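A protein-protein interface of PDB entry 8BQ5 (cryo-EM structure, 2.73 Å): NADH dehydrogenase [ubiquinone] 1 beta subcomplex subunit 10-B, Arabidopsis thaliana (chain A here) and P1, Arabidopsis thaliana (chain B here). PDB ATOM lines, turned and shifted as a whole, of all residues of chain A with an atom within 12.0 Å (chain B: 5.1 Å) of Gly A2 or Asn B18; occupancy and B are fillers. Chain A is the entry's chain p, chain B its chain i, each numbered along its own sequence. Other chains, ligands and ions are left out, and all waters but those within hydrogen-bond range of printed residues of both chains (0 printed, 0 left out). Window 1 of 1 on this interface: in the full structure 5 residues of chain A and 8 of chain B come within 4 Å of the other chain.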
ATOM      1  N   GLY A   2      17.520   0.783  10.400  1.00  0.00           N
ATOM      2  CA  GLY A   2      16.369  -0.092  10.515  1.00  0.00           C
ATOM      3  C   GLY A   2      15.176   0.581  11.165  1.00  0.00           C
ATOM      4  O   GLY A   2      15.335   1.400  12.069  1.00  0.00           O
ATOM      5  N   ARG A   3      13.978   0.235  10.702  1.00  0.00           N
ATOM      6  CA  ARG A   3      12.738   0.799  11.217  1.00  0.00           C
ATOM      7  C   ARG A   3      11.868  -0.306  11.798  1.00  0.00           C
ATOM      8  O   ARG A   3      11.758  -1.392  11.222  1.00  0.00           O
ATOM      9  CB  ARG A   3      11.969   1.554  10.120  1.00  0.00           C
ATOM     10  CG  ARG A   3      10.451   1.480  10.256  1.00  0.00           C
ATOM     11  CD  ARG A   3       9.737   1.955   9.002  1.00  0.00           C
ATOM     12  NE  ARG A   3       9.691   3.409   8.917  1.00  0.00           N
ATOM     13  CZ  ARG A   3       8.764   4.165   9.493  1.00  0.00           C
ATOM     14  NH1 ARG A   3       7.775   3.634  10.192  1.00  0.00           N
ATOM     15  NH2 ARG A   3       8.831   5.486   9.362  1.00  0.00           N
ATOM     16  N   LYS A   4      11.256  -0.020  12.945  1.00  0.00           N
ATOM     17  CA  LYS A   4      10.373  -0.975  13.598  1.00  0.00           C
ATOM     18  C   LYS A   4       9.085  -1.160  12.799  1.00  0.00           C
ATOM     19  O   LYS A   4       8.591  -0.236  12.147  1.00  0.00           O
ATOM     20  CB  LYS A   4      10.051  -0.506  15.017  1.00  0.00           C
ATOM     21  CG  LYS A   4      11.273  -0.398  15.922  1.00  0.00           C
ATOM     22  CD  LYS A   4      10.889  -0.340  17.394  1.00  0.00           C
ATOM     23  CE  LYS A   4      12.126  -0.228  18.275  1.00  0.00           C
ATOM     24  NZ  LYS A   4      11.793  -0.083  19.720  1.00  0.00           N
ATOM     25  N   LYS A   5       8.542  -2.372  12.858  1.00  0.00           N
ATOM     26  CA  LYS A   5       7.315  -2.685  12.136  1.00  0.00           C
ATOM     27  C   LYS A   5       6.119  -1.979  12.768  1.00  0.00           C
ATOM     28  O   LYS A   5       5.966  -1.959  13.992  1.00  0.00           O
ATOM     29  CB  LYS A   5       7.094  -4.197  12.123  1.00  0.00           C
ATOM     30  CG  LYS A   5       5.864  -4.665  11.366  1.00  0.00           C
ATOM     31  CD  LYS A   5       5.534  -6.102  11.736  1.00  0.00           C
ATOM     32  CE  LYS A   5       5.200  -6.933  10.510  1.00  0.00           C
ATOM     33  NZ  LYS A   5       6.325  -6.963   9.536  1.00  0.00           N
ATOM     34  N   GLY A   6       5.275  -1.396  11.927  1.00  0.00           N
ATOM     35  CA  GLY A   6       4.076  -0.716  12.375  1.00  0.00           C
ATOM     36  C   GLY A   6       3.838   0.580  11.623  1.00  0.00           C
ATOM     37  O   GLY A   6       4.626   1.007  10.781  1.00  0.00           O
ATOM     38  N   LEU A   7       2.708   1.202  11.953  1.00  0.00           N
ATOM     39  CA  LEU A   7       2.360   2.491  11.378  1.00  0.00           C
ATOM     40  C   LEU A   7       3.272   3.580  11.942  1.00  0.00           C
ATOM     41  O   LEU A   7       3.849   3.419  13.021  1.00  0.00           O
ATOM     42  CB  LEU A   7       0.899   2.831  11.673  1.00  0.00           C
ATOM     43  CG  LEU A   7      -0.173   1.959  11.019  1.00  0.00           C
ATOM     44  CD1 LEU A   7      -0.543   0.796  11.924  1.00  0.00           C
ATOM     45  CD2 LEU A   7      -1.405   2.789  10.675  1.00  0.00           C
ATOM     46  N   PRO A   8       3.443   4.690  11.221  1.00  0.00           N
ATOM     47  CA  PRO A   8       4.219   5.802  11.780  1.00  0.00           C
ATOM     48  C   PRO A   8       3.501   6.434  12.962  1.00  0.00           C
ATOM     49  O   PRO A   8       2.271   6.485  13.019  1.00  0.00           O
ATOM     50  CB  PRO A   8       4.348   6.787  10.611  1.00  0.00           C
ATOM     51  CG  PRO A   8       3.354   6.377   9.603  1.00  0.00           C
ATOM     52  CD  PRO A   8       2.875   4.995   9.896  1.00  0.00           C
ATOM     53  N   GLU A   9       4.291   6.916  13.914  1.00  0.00           N
ATOM     54  CA  GLU A   9       3.783   7.580  15.107  1.00  0.00           C
ATOM     55  C   GLU A   9       4.239   9.031  15.096  1.00  0.00           C
ATOM     56  O   GLU A   9       5.402   9.317  14.795  1.00  0.00           O
ATOM     57  CB  GLU A   9       4.279   6.886  16.376  1.00  0.00           C
ATOM     58  CG  GLU A   9       3.781   5.465  16.564  1.00  0.00           C
ATOM     59  CD  GLU A   9       2.742   5.345  17.663  1.00  0.00           C
ATOM     60  OE1 GLU A   9       2.408   6.373  18.287  1.00  0.00           O
ATOM     61  OE2 GLU A   9       2.268   4.216  17.908  1.00  0.00           O
ATOM     62  N   PHE A  10       3.326   9.941  15.421  1.00  0.00           N
ATOM     63  CA  PHE A  10       3.655  11.350  15.547  1.00  0.00           C
ATOM     64  C   PHE A  10       3.047  11.899  16.827  1.00  0.00           C
ATOM     65  O   PHE A  10       2.066  11.367  17.353  1.00  0.00           O
ATOM     66  CB  PHE A  10       3.169  12.170  14.345  1.00  0.00           C
ATOM     67  CG  PHE A  10       3.653  11.656  13.022  1.00  0.00           C
ATOM     68  CD1 PHE A  10       4.813  12.157  12.455  1.00  0.00           C
ATOM     69  CD2 PHE A  10       2.942  10.688  12.336  1.00  0.00           C
ATOM     70  CE1 PHE A  10       5.265  11.690  11.238  1.00  0.00           C
ATOM     71  CE2 PHE A  10       3.387  10.219  11.115  1.00  0.00           C
ATOM     72  CZ  PHE A  10       4.551  10.721  10.566  1.00  0.00           C
ATOM     73  N   LEU B  13      12.563  -3.535   5.939  1.00  0.00           N
ATOM     74  CA  LEU B  13      12.601  -2.813   7.207  1.00  0.00           C
ATOM     75  C   LEU B  13      14.033  -2.519   7.646  1.00  0.00           C
ATOM     76  O   LEU B  13      14.298  -1.470   8.244  1.00  0.00           O
ATOM     77  CB  LEU B  13      11.855  -3.610   8.277  1.00  0.00           C
ATOM     78  CG  LEU B  13      10.335  -3.419   8.322  1.00  0.00           C
ATOM     79  CD1 LEU B  13       9.773  -3.887   9.649  1.00  0.00           C
ATOM     80  CD2 LEU B  13       9.963  -1.967   8.070  1.00  0.00           C
ATOM     81  N   ARG B  14      14.974  -3.429   7.369  1.00  0.00           N
ATOM     82  CA  ARG B  14      16.366  -3.167   7.730  1.00  0.00           C
ATOM     83  C   ARG B  14      16.981  -2.088   6.847  1.00  0.00           C
ATOM     84  O   ARG B  14      17.989  -1.475   7.218  1.00  0.00           O
ATOM     85  CB  ARG B  14      17.214  -4.439   7.650  1.00  0.00           C
ATOM     86  CG  ARG B  14      16.903  -5.527   8.651  1.00  0.00           C
ATOM     87  CD  ARG B  14      17.859  -6.696   8.472  1.00  0.00           C
ATOM     88  NE  ARG B  14      17.549  -7.798   9.375  1.00  0.00           N
ATOM     89  CZ  ARG B  14      18.148  -8.981   9.353  1.00  0.00           C
ATOM     90  NH1 ARG B  14      19.102  -9.256   8.478  1.00  0.00           N
ATOM     91  NH2 ARG B  14      17.779  -9.913  10.227  1.00  0.00           N
ATOM     92  N   MET B  16      15.469   0.715   5.799  1.00  0.00           N
ATOM     93  CA  MET B  16      14.913   2.044   6.011  1.00  0.00           C
ATOM     94  C   MET B  16      15.548   2.697   7.231  1.00  0.00           C
ATOM     95  O   MET B  16      15.652   2.084   8.296  1.00  0.00           O
ATOM     96  CB  MET B  16      13.399   1.960   6.188  1.00  0.00           C
ATOM     97  CG  MET B  16      12.693   1.198   5.085  1.00  0.00           C
ATOM     98  SD  MET B  16      10.914   1.055   5.327  1.00  0.00           S
ATOM     99  CE  MET B  16      10.330   2.458   4.386  1.00  0.00           C
ATOM    100  N   GLU B  17      15.912   3.971   7.077  1.00  0.00           N
ATOM    101  CA  GLU B  17      16.505   4.719   8.216  1.00  0.00           C
ATOM    102  C   GLU B  17      15.494   4.783   9.368  1.00  0.00           C
ATOM    103  O   GLU B  17      14.283   4.844   9.097  1.00  0.00           O
ATOM    104  CB  GLU B  17      17.003   6.096   7.764  1.00  0.00           C
ATOM    105  CG  GLU B  17      16.038   6.875   6.900  1.00  0.00           C
ATOM    106  CD  GLU B  17      16.596   8.202   6.415  1.00  0.00           C
ATOM    107  OE1 GLU B  17      17.800   8.454   6.616  1.00  0.00           O
ATOM    108  OE2 GLU B  17      15.824   8.980   5.840  1.00  0.00           O
ATOM    109  N   ASN B  18      15.988   4.757  10.607  1.00  0.00           N
ATOM    110  CA  ASN B  18      15.109   4.783  11.802  1.00  0.00           C
ATOM    111  C   ASN B  18      14.470   6.164  11.900  1.00  0.00           C
ATOM    112  O   ASN B  18      15.211   7.163  11.877  1.00  0.00           O
ATOM    113  CB  ASN B  18      15.888   4.428  13.075  1.00  0.00           C
ATOM    114  CG  ASN B  18      15.041   4.485  14.327  1.00  0.00           C
ATOM    115  OD1 ASN B  18      15.211   5.372  15.159  1.00  0.00           O
ATOM    116  ND2 ASN B  18      14.123   3.543  14.469  1.00  0.00           N
ATOM    117  N   PRO B  19      13.132   6.271  12.007  1.00  0.00           N
ATOM    118  CA  PRO B  19      12.496   7.582  12.016  1.00  0.00           C
ATOM    119  C   PRO B  19      13.056   8.496  13.118  1.00  0.00           C
ATOM    120  O   PRO B  19      13.405   9.613  12.805  1.00  0.00           O
ATOM    121  CB  PRO B  19      11.025   7.247  12.288  1.00  0.00           C
ATOM    122  CG  PRO B  19      10.860   5.817  11.835  1.00  0.00           C
ATOM    123  CD  PRO B  19      12.195   5.156  12.091  1.00  0.00           C
ATOM    124  N   GLU B  20      13.156   8.007  14.358  1.00  0.00           N
ATOM    125  CA  GLU B  20      13.585   8.869  15.496  1.00  0.00           C
ATOM    126  C   GLU B  20      14.997   9.406  15.262  1.00  0.00           C
ATOM    127  O   GLU B  20      15.218  10.604  15.499  1.00  0.00           O
ATOM    128  CB  GLU B  20      13.538   8.072  16.799  1.00  0.00           C
ATOM    129  CG  GLU B  20      12.267   7.258  16.952  1.00  0.00           C
ATOM    130  CD  GLU B  20      10.991   8.080  17.011  1.00  0.00           C
ATOM    131  OE1 GLU B  20       9.959   7.594  16.512  1.00  0.00           O
ATOM    132  OE2 GLU B  20      11.029   9.198  17.565  1.00  0.00           O
ATOM    133  N   GLU B  21      15.907   8.543  14.819  1.00  0.00           N
ATOM    134  CA  GLU B  21      17.313   8.963  14.588  1.00  0.00           C
ATOM    135  C   GLU B  21      17.319  10.048  13.514  1.00  0.00           C
ATOM    136  O   GLU B  21      18.009  11.066  13.725  1.00  0.00           O
ATOM    137  CB  GLU B  21      18.137   7.739  14.202  1.00  0.00           C
ATOM    138  CG  GLU B  21      18.275   6.745  15.340  1.00  0.00           C
ATOM    139  CD  GLU B  21      18.955   5.429  15.001  1.00  0.00           C
ATOM    140  OE1 GLU B  21      19.596   5.349  13.931  1.00  0.00           O
ATOM    141  OE2 GLU B  21      18.841   4.486  15.813  1.00  0.00           O
ATOM    142  N   ARG B  22      16.554   9.855  12.437  1.00  0.00           N
ATOM    143  CA  ARG B  22      16.487  10.854  11.340  1.00  0.00           C
ATOM    144  C   ARG B  22      15.947  12.183  11.874  1.00  0.00           C
ATOM    145  O   ARG B  22      16.640  13.199  11.714  1.00  0.00           O
ATOM    146  CB  ARG B  22      15.574  10.352  10.222  1.00  0.00           C
ATOM    147  CG  ARG B  22      15.722  11.106   8.909  1.00  0.00           C
ATOM    148  CD  ARG B  22      14.411  11.262   8.164  1.00  0.00           C
ATOM    149  NE  ARG B  22      13.799   9.976   7.857  1.00  0.00           N
ATOM    150  CZ  ARG B  22      12.676   9.525   8.400  1.00  0.00           C
ATOM    151  NH1 ARG B  22      12.026  10.259   9.288  1.00  0.00           N
ATOM    152  NH2 ARG B  22      12.207   8.339   8.057  1.00  0.00           N
ATOM    153  N   ASP B  23      14.763  12.162  12.486  1.00  0.00           N
ATOM    154  CA  ASP B  23      14.108  13.408  12.965  1.00  0.00           C
ATOM    155  C   ASP B  23      15.014  14.184  13.925  1.00  0.00           C
ATOM    156  O   ASP B  23      14.963  15.408  13.880  1.00  0.00           O
ATOM    157  CB  ASP B  23      12.741  13.104  13.582  1.00  0.00           C
ATOM    158  CG  ASP B  23      11.761  12.507  12.582  1.00  0.00           C
ATOM    159  OD1 ASP B  23      12.003  12.647  11.364  1.00  0.00           O
ATOM    160  OD2 ASP B  23      10.764  11.908  13.030  1.00  0.00           O
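O of Leu B13 sits at hydrogen-bond distance from N of Arg A3. The backbone carbonyl oxygen (O) of Met B16 lies within hydrogen-bond range of the backbone NH (N) of Gly A2 (3.1 Å). The backbone NH (N) of Arg A3 lies within hydrogen-bond range of the backbone carbonyl oxygen (O) of Met B16, at 3.5 Å. ND2 of Asn B18 sits close to O of Gly A2 (3.4 Å).
The backbone NH (N) of Glu B20 sits close to the side-chain amide oxygen (OD1) of Asn B18, at 3.4 Å. The side-chain amide oxygen (OD1) of Asn B18 sits at hydrogen-bond distance from the backbone NH (N) of Glu B21.
Among the printed residues, merely in contact across the chains: Gly A2 with Leu B13, Gly A2 with Arg B14, Arg A3 with Pro B19 and Lys A5 with Leu B13.
Gly A2 touches four residues of chain B. Printed residues of chain B within 4 Å of Lys A5: Leu B13. Leu A7 touches none of the printed residues of chain B. Of chain A, only Gly A2, Arg A3 and Lys A5 come within 4 Å of Leu B13. Printed residues of chain A within 4 Å of Met B16: Gly A2 and Arg A3. Asn B18 touches just one residue of chain A: Gly A2 (3.2 Å). No residue of chain A comes within 4 Å of Glu B20. No residue of chain A comes within 4 Å of Glu B21. No residue of chain A comes within 4 Å of Arg B22. Asp B23 touches none of the printed residues of chain A. The nearest residue of chain B that does not touch Gly A2 is Glu B17 (4.3 Å). The nearest residue of chain A that does not touch Asn B18 is Arg A3 (4.5 Å).
Hydrophobic or aromatic side chains of chain B that line the printed part of chain A: Leu B13, Met B16 and Pro B19. Of the 9 printed residues of chain A, 3 touch a printed residue of chain B. Among the printed residues, 8 pairs touch across the chains.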
